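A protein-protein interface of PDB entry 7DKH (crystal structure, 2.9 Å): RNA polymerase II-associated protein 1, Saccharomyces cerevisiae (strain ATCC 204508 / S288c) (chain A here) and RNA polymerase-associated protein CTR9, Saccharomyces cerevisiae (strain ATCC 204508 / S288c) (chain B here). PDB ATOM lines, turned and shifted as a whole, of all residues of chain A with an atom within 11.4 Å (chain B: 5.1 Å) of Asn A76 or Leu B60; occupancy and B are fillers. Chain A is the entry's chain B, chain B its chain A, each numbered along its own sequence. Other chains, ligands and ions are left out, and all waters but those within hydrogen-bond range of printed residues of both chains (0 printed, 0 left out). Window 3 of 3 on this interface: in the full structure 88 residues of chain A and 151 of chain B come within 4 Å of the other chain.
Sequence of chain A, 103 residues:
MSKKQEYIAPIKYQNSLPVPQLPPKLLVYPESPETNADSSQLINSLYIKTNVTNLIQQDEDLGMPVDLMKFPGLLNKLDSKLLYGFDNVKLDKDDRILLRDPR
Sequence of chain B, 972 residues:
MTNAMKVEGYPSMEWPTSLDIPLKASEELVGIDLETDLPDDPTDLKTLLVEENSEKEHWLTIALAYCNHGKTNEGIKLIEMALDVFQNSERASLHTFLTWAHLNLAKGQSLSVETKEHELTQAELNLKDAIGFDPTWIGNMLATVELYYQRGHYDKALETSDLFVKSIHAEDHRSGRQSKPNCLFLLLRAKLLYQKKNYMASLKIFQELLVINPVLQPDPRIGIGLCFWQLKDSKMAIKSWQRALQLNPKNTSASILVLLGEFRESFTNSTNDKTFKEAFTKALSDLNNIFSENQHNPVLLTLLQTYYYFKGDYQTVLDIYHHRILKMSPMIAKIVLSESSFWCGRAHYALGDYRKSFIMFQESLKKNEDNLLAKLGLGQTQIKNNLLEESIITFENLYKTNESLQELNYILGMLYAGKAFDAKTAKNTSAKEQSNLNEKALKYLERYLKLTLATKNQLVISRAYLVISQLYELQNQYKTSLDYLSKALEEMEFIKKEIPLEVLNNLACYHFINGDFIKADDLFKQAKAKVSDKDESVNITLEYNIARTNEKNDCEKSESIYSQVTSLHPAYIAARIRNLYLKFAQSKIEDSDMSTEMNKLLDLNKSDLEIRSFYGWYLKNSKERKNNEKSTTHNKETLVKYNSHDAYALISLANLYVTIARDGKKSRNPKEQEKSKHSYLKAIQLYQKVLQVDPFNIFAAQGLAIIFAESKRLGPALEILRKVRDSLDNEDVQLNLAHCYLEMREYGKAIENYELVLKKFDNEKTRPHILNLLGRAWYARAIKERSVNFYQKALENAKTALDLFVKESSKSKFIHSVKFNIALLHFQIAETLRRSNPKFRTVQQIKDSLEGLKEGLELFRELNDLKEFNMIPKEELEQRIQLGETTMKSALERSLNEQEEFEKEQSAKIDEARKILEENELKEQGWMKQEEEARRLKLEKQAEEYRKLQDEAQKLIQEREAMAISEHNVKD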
ATOM      1  N   LEU A  68       7.684   6.015  19.867  1.00  0.00           N
ATOM      2  CA  LEU A  68       8.946   5.577  20.459  1.00  0.00           C
ATOM      3  C   LEU A  68       9.787   4.741  19.509  1.00  0.00           C
ATOM      4  O   LEU A  68      10.922   4.399  19.852  1.00  0.00           O
ATOM      5  CB  LEU A  68       8.713   4.784  21.751  1.00  0.00           C
ATOM      6  CG  LEU A  68       8.837   5.619  23.031  1.00  0.00           C
ATOM      7  CD1 LEU A  68       7.911   6.825  22.990  1.00  0.00           C
ATOM      8  CD2 LEU A  68       8.616   4.797  24.295  1.00  0.00           C
ATOM      9  N   MET A  69       9.262   4.404  18.338  1.00  0.00           N
ATOM     10  CA  MET A  69       9.980   3.560  17.396  1.00  0.00           C
ATOM     11  C   MET A  69      10.931   4.421  16.565  1.00  0.00           C
ATOM     12  O   MET A  69      11.664   3.931  15.703  1.00  0.00           O
ATOM     13  CB  MET A  69       8.977   2.811  16.524  1.00  0.00           C
ATOM     14  CG  MET A  69       8.394   1.605  17.227  1.00  0.00           C
ATOM     15  SD  MET A  69       7.357   0.477  16.047  1.00  0.00           S
ATOM     16  CE  MET A  69       5.603   1.118  16.555  1.00  0.00           C
ATOM     17  N   LYS A  70      10.902   5.721  16.862  1.00  0.00           N
ATOM     18  CA  LYS A  70      11.742   6.737  16.245  1.00  0.00           C
ATOM     19  C   LYS A  70      13.046   6.960  17.003  1.00  0.00           C
ATOM     20  O   LYS A  70      13.847   7.808  16.596  1.00  0.00           O
ATOM     21  CB  LYS A  70      10.992   8.079  16.198  1.00  0.00           C
ATOM     22  CG  LYS A  70       9.728   8.197  15.334  1.00  0.00           C
ATOM     23  CD  LYS A  70       9.998   8.289  13.836  1.00  0.00           C
ATOM     24  CE  LYS A  70       8.682   8.357  13.055  1.00  0.00           C
ATOM     25  NZ  LYS A  70       8.862   8.328  11.573  1.00  0.00           N
ATOM     26  N   PHE A  71      13.277   6.228  18.092  1.00  0.00           N
ATOM     27  CA  PHE A  71      14.453   6.428  18.942  1.00  0.00           C
ATOM     28  C   PHE A  71      15.355   5.202  18.915  1.00  0.00           C
ATOM     29  O   PHE A  71      15.043   4.183  19.557  1.00  0.00           O
ATOM     30  CB  PHE A  71      14.032   6.754  20.376  1.00  0.00           C
ATOM     31  CG  PHE A  71      13.269   8.052  20.505  1.00  0.00           C
ATOM     32  CD1 PHE A  71      11.894   8.081  20.326  1.00  0.00           C
ATOM     33  CD2 PHE A  71      13.926   9.238  20.800  1.00  0.00           C
ATOM     34  CE1 PHE A  71      11.189   9.267  20.439  1.00  0.00           C
ATOM     35  CE2 PHE A  71      13.222  10.427  20.916  1.00  0.00           C
ATOM     36  CZ  PHE A  71      11.852  10.441  20.735  1.00  0.00           C
ATOM     37  N   PRO A  72      16.463   5.249  18.175  1.00  0.00           N
ATOM     38  CA  PRO A  72      17.367   4.095  18.112  1.00  0.00           C
ATOM     39  C   PRO A  72      17.939   3.744  19.478  1.00  0.00           C
ATOM     40  O   PRO A  72      18.197   4.614  20.311  1.00  0.00           O
ATOM     41  CB  PRO A  72      18.463   4.560  17.145  1.00  0.00           C
ATOM     42  CG  PRO A  72      17.786   5.578  16.292  1.00  0.00           C
ATOM     43  CD  PRO A  72      16.828   6.290  17.202  1.00  0.00           C
ATOM     44  N   GLY A  73      18.132   2.456  19.698  1.00  0.00           N
ATOM     45  CA  GLY A  73      18.621   1.959  20.979  1.00  0.00           C
ATOM     46  C   GLY A  73      17.497   1.660  21.941  1.00  0.00           C
ATOM     47  O   GLY A  73      17.467   0.595  22.557  1.00  0.00           O
ATOM     48  N   LEU A  74      16.570   2.602  22.086  1.00  0.00           N
ATOM     49  CA  LEU A  74      15.382   2.396  22.897  1.00  0.00           C
ATOM     50  C   LEU A  74      14.375   1.528  22.155  1.00  0.00           C
ATOM     51  O   LEU A  74      14.245   1.611  20.929  1.00  0.00           O
ATOM     52  CB  LEU A  74      14.756   3.747  23.261  1.00  0.00           C
ATOM     53  CG  LEU A  74      13.412   3.818  23.996  1.00  0.00           C
ATOM     54  CD1 LEU A  74      13.452   4.911  25.042  1.00  0.00           C
ATOM     55  CD2 LEU A  74      12.259   4.065  23.040  1.00  0.00           C
ATOM     56  N   LEU A  75      13.682   0.678  22.912  1.00  0.00           N
ATOM     57  CA  LEU A  75      12.706  -0.325  22.503  1.00  0.00           C
ATOM     58  C   LEU A  75      13.364  -1.581  21.939  1.00  0.00           C
ATOM     59  O   LEU A  75      12.671  -2.577  21.741  1.00  0.00           O
ATOM     60  CB  LEU A  75      11.686   0.198  21.470  1.00  0.00           C
ATOM     61  CG  LEU A  75      10.507   1.031  21.985  1.00  0.00           C
ATOM     62  CD1 LEU A  75       9.330   0.968  21.023  1.00  0.00           C
ATOM     63  CD2 LEU A  75      10.087   0.642  23.398  1.00  0.00           C
ATOM     64  N   ASN A  76      14.663  -1.580  21.665  1.00  0.00           N
ATOM     65  CA  ASN A  76      15.351  -2.815  21.295  1.00  0.00           C
ATOM     66  C   ASN A  76      16.519  -3.141  22.211  1.00  0.00           C
ATOM     67  O   ASN A  76      16.680  -4.300  22.596  1.00  0.00           O
ATOM     68  CB  ASN A  76      15.821  -2.774  19.829  1.00  0.00           C
ATOM     69  CG  ASN A  76      16.785  -1.649  19.547  1.00  0.00           C
ATOM     70  OD1 ASN A  76      16.742  -0.603  20.186  1.00  0.00           O
ATOM     71  ND2 ASN A  76      17.657  -1.853  18.561  1.00  0.00           N
ATOM     72  N   LYS A  77      17.351  -2.153  22.551  1.00  0.00           N
ATOM     73  CA  LYS A  77      18.482  -2.342  23.449  1.00  0.00           C
ATOM     74  C   LYS A  77      18.245  -1.737  24.827  1.00  0.00           C
ATOM     75  O   LYS A  77      19.166  -1.731  25.652  1.00  0.00           O
ATOM     76  CB  LYS A  77      19.753  -1.725  22.847  1.00  0.00           C
ATOM     77  CG  LYS A  77      20.081  -2.142  21.424  1.00  0.00           C
ATOM     78  CD  LYS A  77      21.170  -1.237  20.858  1.00  0.00           C
ATOM     79  CE  LYS A  77      21.301  -1.371  19.350  1.00  0.00           C
ATOM     80  NZ  LYS A  77      21.800  -2.712  18.943  1.00  0.00           N
ATOM     81  N   LEU A  78      17.044  -1.211  25.088  1.00  0.00           N
ATOM     82  CA  LEU A  78      16.691  -0.602  26.376  1.00  0.00           C
ATOM     83  C   LEU A  78      17.551   0.631  26.658  1.00  0.00           C
ATOM     84  O   LEU A  78      17.977   0.870  27.790  1.00  0.00           O
ATOM     85  CB  LEU A  78      16.779  -1.608  27.532  1.00  0.00           C
ATOM     86  CG  LEU A  78      15.734  -2.728  27.657  1.00  0.00           C
ATOM     87  CD1 LEU A  78      14.299  -2.195  27.615  1.00  0.00           C
ATOM     88  CD2 LEU A  78      15.940  -3.820  26.620  1.00  0.00           C
ATOM     89  N   ASP A  79      17.807   1.422  25.615  1.00  0.00           N
ATOM     90  CA  ASP A  79      18.745   2.548  25.672  1.00  0.00           C
ATOM     91  C   ASP A  79      17.981   3.868  25.785  1.00  0.00           C
ATOM     92  O   ASP A  79      17.700   4.534  24.787  1.00  0.00           O
ATOM     93  CB  ASP A  79      19.656   2.540  24.451  1.00  0.00           C
ATOM     94  CG  ASP A  79      20.902   3.374  24.647  1.00  0.00           C
ATOM     95  OD1 ASP A  79      20.975   4.106  25.657  1.00  0.00           O
ATOM     96  OD2 ASP A  79      21.807   3.309  23.788  1.00  0.00           O
ATOM     97  N   SER A  80      17.635   4.245  27.018  1.00  0.00           N
ATOM     98  CA  SER A  80      16.894   5.472  27.303  1.00  0.00           C
ATOM     99  C   SER A  80      17.652   6.747  26.932  1.00  0.00           C
ATOM    100  O   SER A  80      17.070   7.834  27.026  1.00  0.00           O
ATOM    101  CB  SER A  80      16.499   5.520  28.778  1.00  0.00           C
ATOM    102  OG  SER A  80      17.398   6.318  29.527  1.00  0.00           O
ATOM    103  N   LYS A  81      18.922   6.643  26.529  1.00  0.00           N
ATOM    104  CA  LYS A  81      19.768   7.824  26.357  1.00  0.00           C
ATOM    105  C   LYS A  81      19.175   8.838  25.386  1.00  0.00           C
ATOM    106  O   LYS A  81      19.179  10.043  25.663  1.00  0.00           O
ATOM    107  CB  LYS A  81      21.155   7.390  25.878  1.00  0.00           C
ATOM    108  CG  LYS A  81      22.175   8.507  25.715  1.00  0.00           C
ATOM    109  CD  LYS A  81      22.318   9.419  26.911  1.00  0.00           C
ATOM    110  CE  LYS A  81      23.575  10.260  26.739  1.00  0.00           C
ATOM    111  NZ  LYS A  81      24.071  10.827  28.013  1.00  0.00           N
ATOM    112  N   LEU A  82      18.658   8.384  24.247  1.00  0.00           N
ATOM    113  CA  LEU A  82      18.266   9.339  23.217  1.00  0.00           C
ATOM    114  C   LEU A  82      17.049  10.180  23.598  1.00  0.00           C
ATOM    115  O   LEU A  82      16.766  11.164  22.908  1.00  0.00           O
ATOM    116  CB  LEU A  82      18.006   8.617  21.894  1.00  0.00           C
ATOM    117  CG  LEU A  82      19.245   8.376  21.024  1.00  0.00           C
ATOM    118  CD1 LEU A  82      18.856   7.883  19.638  1.00  0.00           C
ATOM    119  CD2 LEU A  82      20.126   9.618  20.929  1.00  0.00           C
ATOM    120  N   LEU A  83      16.338   9.844  24.680  1.00  0.00           N
ATOM    121  CA  LEU A  83      15.233  10.682  25.132  1.00  0.00           C
ATOM    122  C   LEU A  83      15.676  11.913  25.905  1.00  0.00           C
ATOM    123  O   LEU A  83      14.866  12.825  26.092  1.00  0.00           O
ATOM    124  CB  LEU A  83      14.278   9.895  26.028  1.00  0.00           C
ATOM    125  CG  LEU A  83      13.770   8.539  25.561  1.00  0.00           C
ATOM    126  CD1 LEU A  83      12.736   8.033  26.552  1.00  0.00           C
ATOM    127  CD2 LEU A  83      13.192   8.625  24.158  1.00  0.00           C
ATOM    128  N   TRP B  15      18.143   5.294  11.811  1.00  0.00           N
ATOM    129  CA  TRP B  15      18.416   3.943  12.281  1.00  0.00           C
ATOM    130  C   TRP B  15      19.510   3.287  11.448  1.00  0.00           C
ATOM    131  O   TRP B  15      19.620   3.544  10.244  1.00  0.00           O
ATOM    132  CB  TRP B  15      17.158   3.081  12.207  1.00  0.00           C
ATOM    133  CG  TRP B  15      16.212   3.264  13.349  1.00  0.00           C
ATOM    134  CD1 TRP B  15      15.228   4.200  13.451  1.00  0.00           C
ATOM    135  CD2 TRP B  15      16.155   2.486  14.551  1.00  0.00           C
ATOM    136  NE1 TRP B  15      14.559   4.056  14.644  1.00  0.00           N
ATOM    137  CE2 TRP B  15      15.110   3.010  15.337  1.00  0.00           C
ATOM    138  CE3 TRP B  15      16.887   1.399  15.040  1.00  0.00           C
ATOM    139  CZ2 TRP B  15      14.775   2.483  16.583  1.00  0.00           C
ATOM    140  CZ3 TRP B  15      16.555   0.879  16.280  1.00  0.00           C
ATOM    141  CH2 TRP B  15      15.509   1.420  17.036  1.00  0.00           C
ATOM    142  N   LYS B  56      17.092 -11.620  21.804  1.00  0.00           N
ATOM    143  CA  LYS B  56      15.788 -10.999  21.588  1.00  0.00           C
ATOM    144  C   LYS B  56      15.915  -9.604  20.992  1.00  0.00           C
ATOM    145  O   LYS B  56      14.967  -9.111  20.359  1.00  0.00           O
ATOM    146  CB  LYS B  56      15.005 -10.922  22.907  1.00  0.00           C
ATOM    147  CG  LYS B  56      15.546  -9.908  23.919  1.00  0.00           C
ATOM    148  CD  LYS B  56      14.428  -9.381  24.810  1.00  0.00           C
ATOM    149  CE  LYS B  56      14.883  -9.075  26.226  1.00  0.00           C
ATOM    150  NZ  LYS B  56      13.747  -8.575  27.057  1.00  0.00           N
ATOM    151  N   GLU B  57      17.076  -8.968  21.170  1.00  0.00           N
ATOM    152  CA  GLU B  57      17.269  -7.617  20.668  1.00  0.00           C
ATOM    153  C   GLU B  57      17.271  -7.585  19.146  1.00  0.00           C
ATOM    154  O   GLU B  57      16.860  -6.584  18.557  1.00  0.00           O
ATOM    155  CB  GLU B  57      18.558  -7.016  21.244  1.00  0.00           C
ATOM    156  CG  GLU B  57      19.848  -7.424  20.551  1.00  0.00           C
ATOM    157  CD  GLU B  57      20.906  -6.330  20.625  1.00  0.00           C
ATOM    158  OE1 GLU B  57      21.377  -6.031  21.744  1.00  0.00           O
ATOM    159  OE2 GLU B  57      21.242  -5.748  19.572  1.00  0.00           O
ATOM    160  N   HIS B  58      17.690  -8.671  18.491  1.00  0.00           N
ATOM    161  CA  HIS B  58      17.671  -8.680  17.029  1.00  0.00           C
ATOM    162  C   HIS B  58      16.263  -8.916  16.491  1.00  0.00           C
ATOM    163  O   HIS B  58      15.890  -8.358  15.451  1.00  0.00           O
ATOM    164  CB  HIS B  58      18.634  -9.735  16.477  1.00  0.00           C
ATOM    165  CG  HIS B  58      20.057  -9.559  16.912  1.00  0.00           C
ATOM    166  ND1 HIS B  58      20.932 -10.616  17.042  1.00  0.00           N
ATOM    167  CD2 HIS B  58      20.764  -8.447  17.227  1.00  0.00           C
ATOM    168  CE1 HIS B  58      22.114 -10.165  17.422  1.00  0.00           C
ATOM    169  NE2 HIS B  58      22.038  -8.852  17.544  1.00  0.00           N
ATOM    170  N   TRP B  59      15.459  -9.720  17.196  1.00  0.00           N
ATOM    171  CA  TRP B  59      14.029  -9.788  16.906  1.00  0.00           C
ATOM    172  C   TRP B  59      13.413  -8.395  16.978  1.00  0.00           C
ATOM    173  O   TRP B  59      12.683  -7.967  16.070  1.00  0.00           O
ATOM    174  CB  TRP B  59      13.332 -10.731  17.892  1.00  0.00           C
ATOM    175  CG  TRP B  59      13.721 -12.193  17.800  1.00  0.00           C
ATOM    176  CD1 TRP B  59      14.895 -12.765  18.209  1.00  0.00           C
ATOM    177  CD2 TRP B  59      12.905 -13.264  17.308  1.00  0.00           C
ATOM    178  NE1 TRP B  59      14.863 -14.121  17.980  1.00  0.00           N
ATOM    179  CE2 TRP B  59      13.654 -14.452  17.430  1.00  0.00           C
ATOM    180  CE3 TRP B  59      11.619 -13.331  16.766  1.00  0.00           C
ATOM    181  CZ2 TRP B  59      13.156 -15.693  17.031  1.00  0.00           C
ATOM    182  CZ3 TRP B  59      11.128 -14.560  16.370  1.00  0.00           C
ATOM    183  CH2 TRP B  59      11.895 -15.725  16.503  1.00  0.00           C
ATOM    184  N   LEU B  60      13.699  -7.676  18.067  1.00  0.00           N
ATOM    185  CA  LEU B  60      13.162  -6.328  18.227  1.00  0.00           C
ATOM    186  C   LEU B  60      13.666  -5.396  17.131  1.00  0.00           C
ATOM    187  O   LEU B  60      12.908  -4.565  16.618  1.00  0.00           O
ATOM    188  CB  LEU B  60      13.527  -5.779  19.606  1.00  0.00           C
ATOM    189  CG  LEU B  60      12.723  -6.315  20.790  1.00  0.00           C
ATOM    190  CD1 LEU B  60      13.398  -5.963  22.102  1.00  0.00           C
ATOM    191  CD2 LEU B  60      11.310  -5.765  20.753  1.00  0.00           C
ATOM    192  N   THR B  61      14.937  -5.532  16.744  1.00  0.00           N
ATOM    193  CA  THR B  61      15.502  -4.652  15.727  1.00  0.00           C
ATOM    194  C   THR B  61      14.846  -4.883  14.371  1.00  0.00           C
ATOM    195  O   THR B  61      14.483  -3.927  13.677  1.00  0.00           O
ATOM    196  CB  THR B  61      17.016  -4.858  15.636  1.00  0.00           C
ATOM    197  OG1 THR B  61      17.636  -4.409  16.848  1.00  0.00           O
ATOM    198  CG2 THR B  61      17.594  -4.082  14.460  1.00  0.00           C
ATOM    199  N   ILE B  62      14.655  -6.148  13.989  1.00  0.00           N
ATOM    200  CA  ILE B  62      14.010  -6.438  12.710  1.00  0.00           C
ATOM    201  C   ILE B  62      12.555  -5.984  12.728  1.00  0.00           C
ATOM    202  O   ILE B  62      12.035  -5.480  11.724  1.00  0.00           O
ATOM    203  CB  ILE B  62      14.134  -7.933  12.364  1.00  0.00           C
ATOM    204  CG1 ILE B  62      15.598  -8.306  12.120  1.00  0.00           C
ATOM    205  CG2 ILE B  62      13.288  -8.282  11.148  1.00  0.00           C
ATOM    206  CD1 ILE B  62      15.876  -9.773  12.315  1.00  0.00           C
ATOM    207  N   ALA B  63      11.877  -6.142  13.866  1.00  0.00           N
ATOM    208  CA  ALA B  63      10.491  -5.689  13.926  1.00  0.00           C
ATOM    209  C   ALA B  63      10.402  -4.173  13.807  1.00  0.00           C
ATOM    210  O   ALA B  63       9.525  -3.644  13.104  1.00  0.00           O
ATOM    211  CB  ALA B  63       9.841  -6.166  15.221  1.00  0.00           C
ATOM    212  N   LEU B  64      11.315  -3.458  14.469  1.00  0.00           N
ATOM    213  CA  LEU B  64      11.332  -2.005  14.359  1.00  0.00           C
ATOM    214  C   LEU B  64      11.648  -1.567  12.936  1.00  0.00           C
ATOM    215  O   LEU B  64      11.113  -0.561  12.458  1.00  0.00           O
ATOM    216  CB  LEU B  64      12.339  -1.415  15.337  1.00  0.00           C
ATOM    217  CG  LEU B  64      11.999  -1.572  16.821  1.00  0.00           C
ATOM    218  CD1 LEU B  64      13.274  -1.549  17.641  1.00  0.00           C
ATOM    219  CD2 LEU B  64      11.051  -0.496  17.277  1.00  0.00           C
ATOM    220  N   ALA B  65      12.534  -2.296  12.254  1.00  0.00           N
ATOM    221  CA  ALA B  65      12.821  -2.001  10.854  1.00  0.00           C
ATOM    222  C   ALA B  65      11.575  -2.168   9.990  1.00  0.00           C
ATOM    223  O   ALA B  65      11.281  -1.328   9.128  1.00  0.00           O
ATOM    224  CB  ALA B  65      13.945  -2.904  10.350  1.00  0.00           C
ATOM    225  N   ILE B  79       7.129 -10.102  16.495  1.00  0.00           N
ATOM    226  CA  ILE B  79       7.282 -10.106  17.949  1.00  0.00           C
ATOM    227  C   ILE B  79       6.200 -10.959  18.601  1.00  0.00           C
ATOM    228  O   ILE B  79       6.398 -11.460  19.715  1.00  0.00           O
ATOM    229  CB  ILE B  79       7.298  -8.671  18.504  1.00  0.00           C
ATOM    230  CG1 ILE B  79       8.467  -7.901  17.894  1.00  0.00           C
ATOM    231  CG2 ILE B  79       7.469  -8.669  20.014  1.00  0.00           C
ATOM    232  CD1 ILE B  79       9.819  -8.271  18.466  1.00  0.00           C
ATOM    233  N   SER B  93      10.299  -6.355  27.742  1.00  0.00           N
ATOM    234  CA  SER B  93      10.554  -5.555  26.547  1.00  0.00           C
ATOM    235  C   SER B  93       9.601  -5.897  25.404  1.00  0.00           C
ATOM    236  O   SER B  93       9.013  -5.003  24.786  1.00  0.00           O
ATOM    237  CB  SER B  93      12.008  -5.727  26.103  1.00  0.00           C
ATOM    238  OG  SER B  93      12.109  -6.661  25.046  1.00  0.00           O
ATOM    239  N   LEU B  94       9.439  -7.193  25.103  1.00  0.00           N
ATOM    240  CA  LEU B  94       8.621  -7.582  23.954  1.00  0.00           C
ATOM    241  C   LEU B  94       7.182  -7.111  24.090  1.00  0.00           C
ATOM    242  O   LEU B  94       6.521  -6.841  23.081  1.00  0.00           O
ATOM    243  CB  LEU B  94       8.650  -9.095  23.737  1.00  0.00           C
ATOM    244  CG  LEU B  94       9.905  -9.762  23.173  1.00  0.00           C
ATOM    245  CD1 LEU B  94      11.101  -9.642  24.086  1.00  0.00           C
ATOM    246  CD2 LEU B  94       9.600 -11.220  22.881  1.00  0.00           C
ATOM    247  N   PHE B  97       7.357  -3.092  23.355  1.00  0.00           N
ATOM    248  CA  PHE B  97       7.334  -2.949  21.905  1.00  0.00           C
ATOM    249  C   PHE B  97       5.915  -3.056  21.379  1.00  0.00           C
ATOM    250  O   PHE B  97       5.400  -2.129  20.742  1.00  0.00           O
ATOM    251  CB  PHE B  97       8.205  -4.015  21.229  1.00  0.00           C
ATOM    252  CG  PHE B  97       8.066  -4.035  19.722  1.00  0.00           C
ATOM    253  CD1 PHE B  97       8.847  -3.205  18.935  1.00  0.00           C
ATOM    254  CD2 PHE B  97       7.136  -4.860  19.096  1.00  0.00           C
ATOM    255  CE1 PHE B  97       8.718  -3.202  17.552  1.00  0.00           C
ATOM    256  CE2 PHE B  97       6.999  -4.855  17.711  1.00  0.00           C
ATOM    257  CZ  PHE B  97       7.793  -4.026  16.941  1.00  0.00           C
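The side-chain hydroxyl (OG1) of Thr B61 is in hydrogen-bond range of the side-chain amide nitrogen (ND2) of Asn A76.
The indole nitrogen (NE1) of Trp B15 sits at hydrogen-bond distance from the backbone carbonyl oxygen (O) of Met A69, at 3.1 Å.
The side-chain carboxylate (OE2) of Glu B57 is in salt-bridge range of the side-chain amino group (NZ) of Lys A77.
The backbone carbonyl oxygen of Gly A73 is in hydrogen-bond range of the backbone NH of Asp A79 (3.2 Å).
The backbone carbonyl oxygen (O) of Gly A73 lies close to the side-chain amide oxygen (OD1) of Asn A76 (2.8 Å).
The backbone carbonyl oxygen of Glu B57 sits at hydrogen-bond distance from the side-chain hydroxyl of Thr B61 (2.9 Å).
The backbone carbonyl oxygen (O) of Leu A74 sits close to the side-chain amide oxygen (OD1) of Asn A76, 3.4 Å away.
The backbone NH of Leu A78 lies within hydrogen-bond range of the backbone carbonyl oxygen of Gly A73 (3.1 Å).
Among the printed residues, pairs that only touch across the chains: Met A69 with Leu B64, Pro A72 with Trp B15, Phe A71 with Trp B15, Leu A75 with Leu B60, Asn A76 with Glu B57, Asn A76 with Leu B64, Asn A76 with Leu B60, Asn A76 with Trp B15 and Gly A73 with Trp B15.
Of the printed residues of chain B, Phe A71 touches Trp B15.
Printed residues of chain B within 4 Å of Pro A72: Trp B15 (3.4 Å).
Of the printed residues of chain B, Gly A73 touches Trp B15 (3.9 Å).
Of chain B, only Trp B15 (3.7 Å), Glu B57 (3.6 Å), Leu B60 (3.7 Å), Thr B61 (3.1 Å) and Leu B64 (3.6 Å) come within 4 Å of Asn A76.
Of the printed residues of chain B, Lys A77 touches Glu B57.
Ser A80 touches none of the printed residues of chain B.
No residue of chain A comes within 4 Å of Lys B56.
Of chain A, only Asn A76 (3.6 Å) and Lys A77 (3.2 Å) come within 4 Å of Glu B57.
Trp B59 touches none of the printed residues of chain A.
Of chain A, only Leu A75 (3.5 Å) and Asn A76 (3.7 Å) come within 4 Å of Leu B60.
Of the printed residues of chain A, Thr B61 touches Asn A76.
No residue of chain A comes within 4 Å of Ile B62.
No residue of chain A comes within 4 Å of Ser B93.
Phe B97 touches none of the printed residues of chain A.
The nearest printed residue of chain A that does not touch Trp B15 is Lys A70 (4.04 Å).
Of the 16 printed residues of chain A, 7 touch a printed residue of chain B.
Printed residues of chain A that touch a printed residue of chain B: Met A69, Phe A71, Pro A72, Gly A73, Leu A75, Asn A76 and Lys A77.
Hydrophobic or aromatic side chains of chain A within 4 Å of the printed part of chain B: Met A69 and Pro A72.
Along chain A the printed residues that touch a printed residue of chain B span positions 69 to 77.
Of the 15 printed residues of chain B, 5 touch a printed residue of chain A.
Printed residues of chain B that touch a printed residue of chain A: Trp B15, Glu B57, Leu B60, Thr B61 and Leu B64.
Among the printed residues, 12 pairs touch across the chains.
Among the printed residues, Asp or Glu carboxylates within 4 Å of a Lys or Arg side-chain nitrogen of the other chain: Lys A77 with Glu B57.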
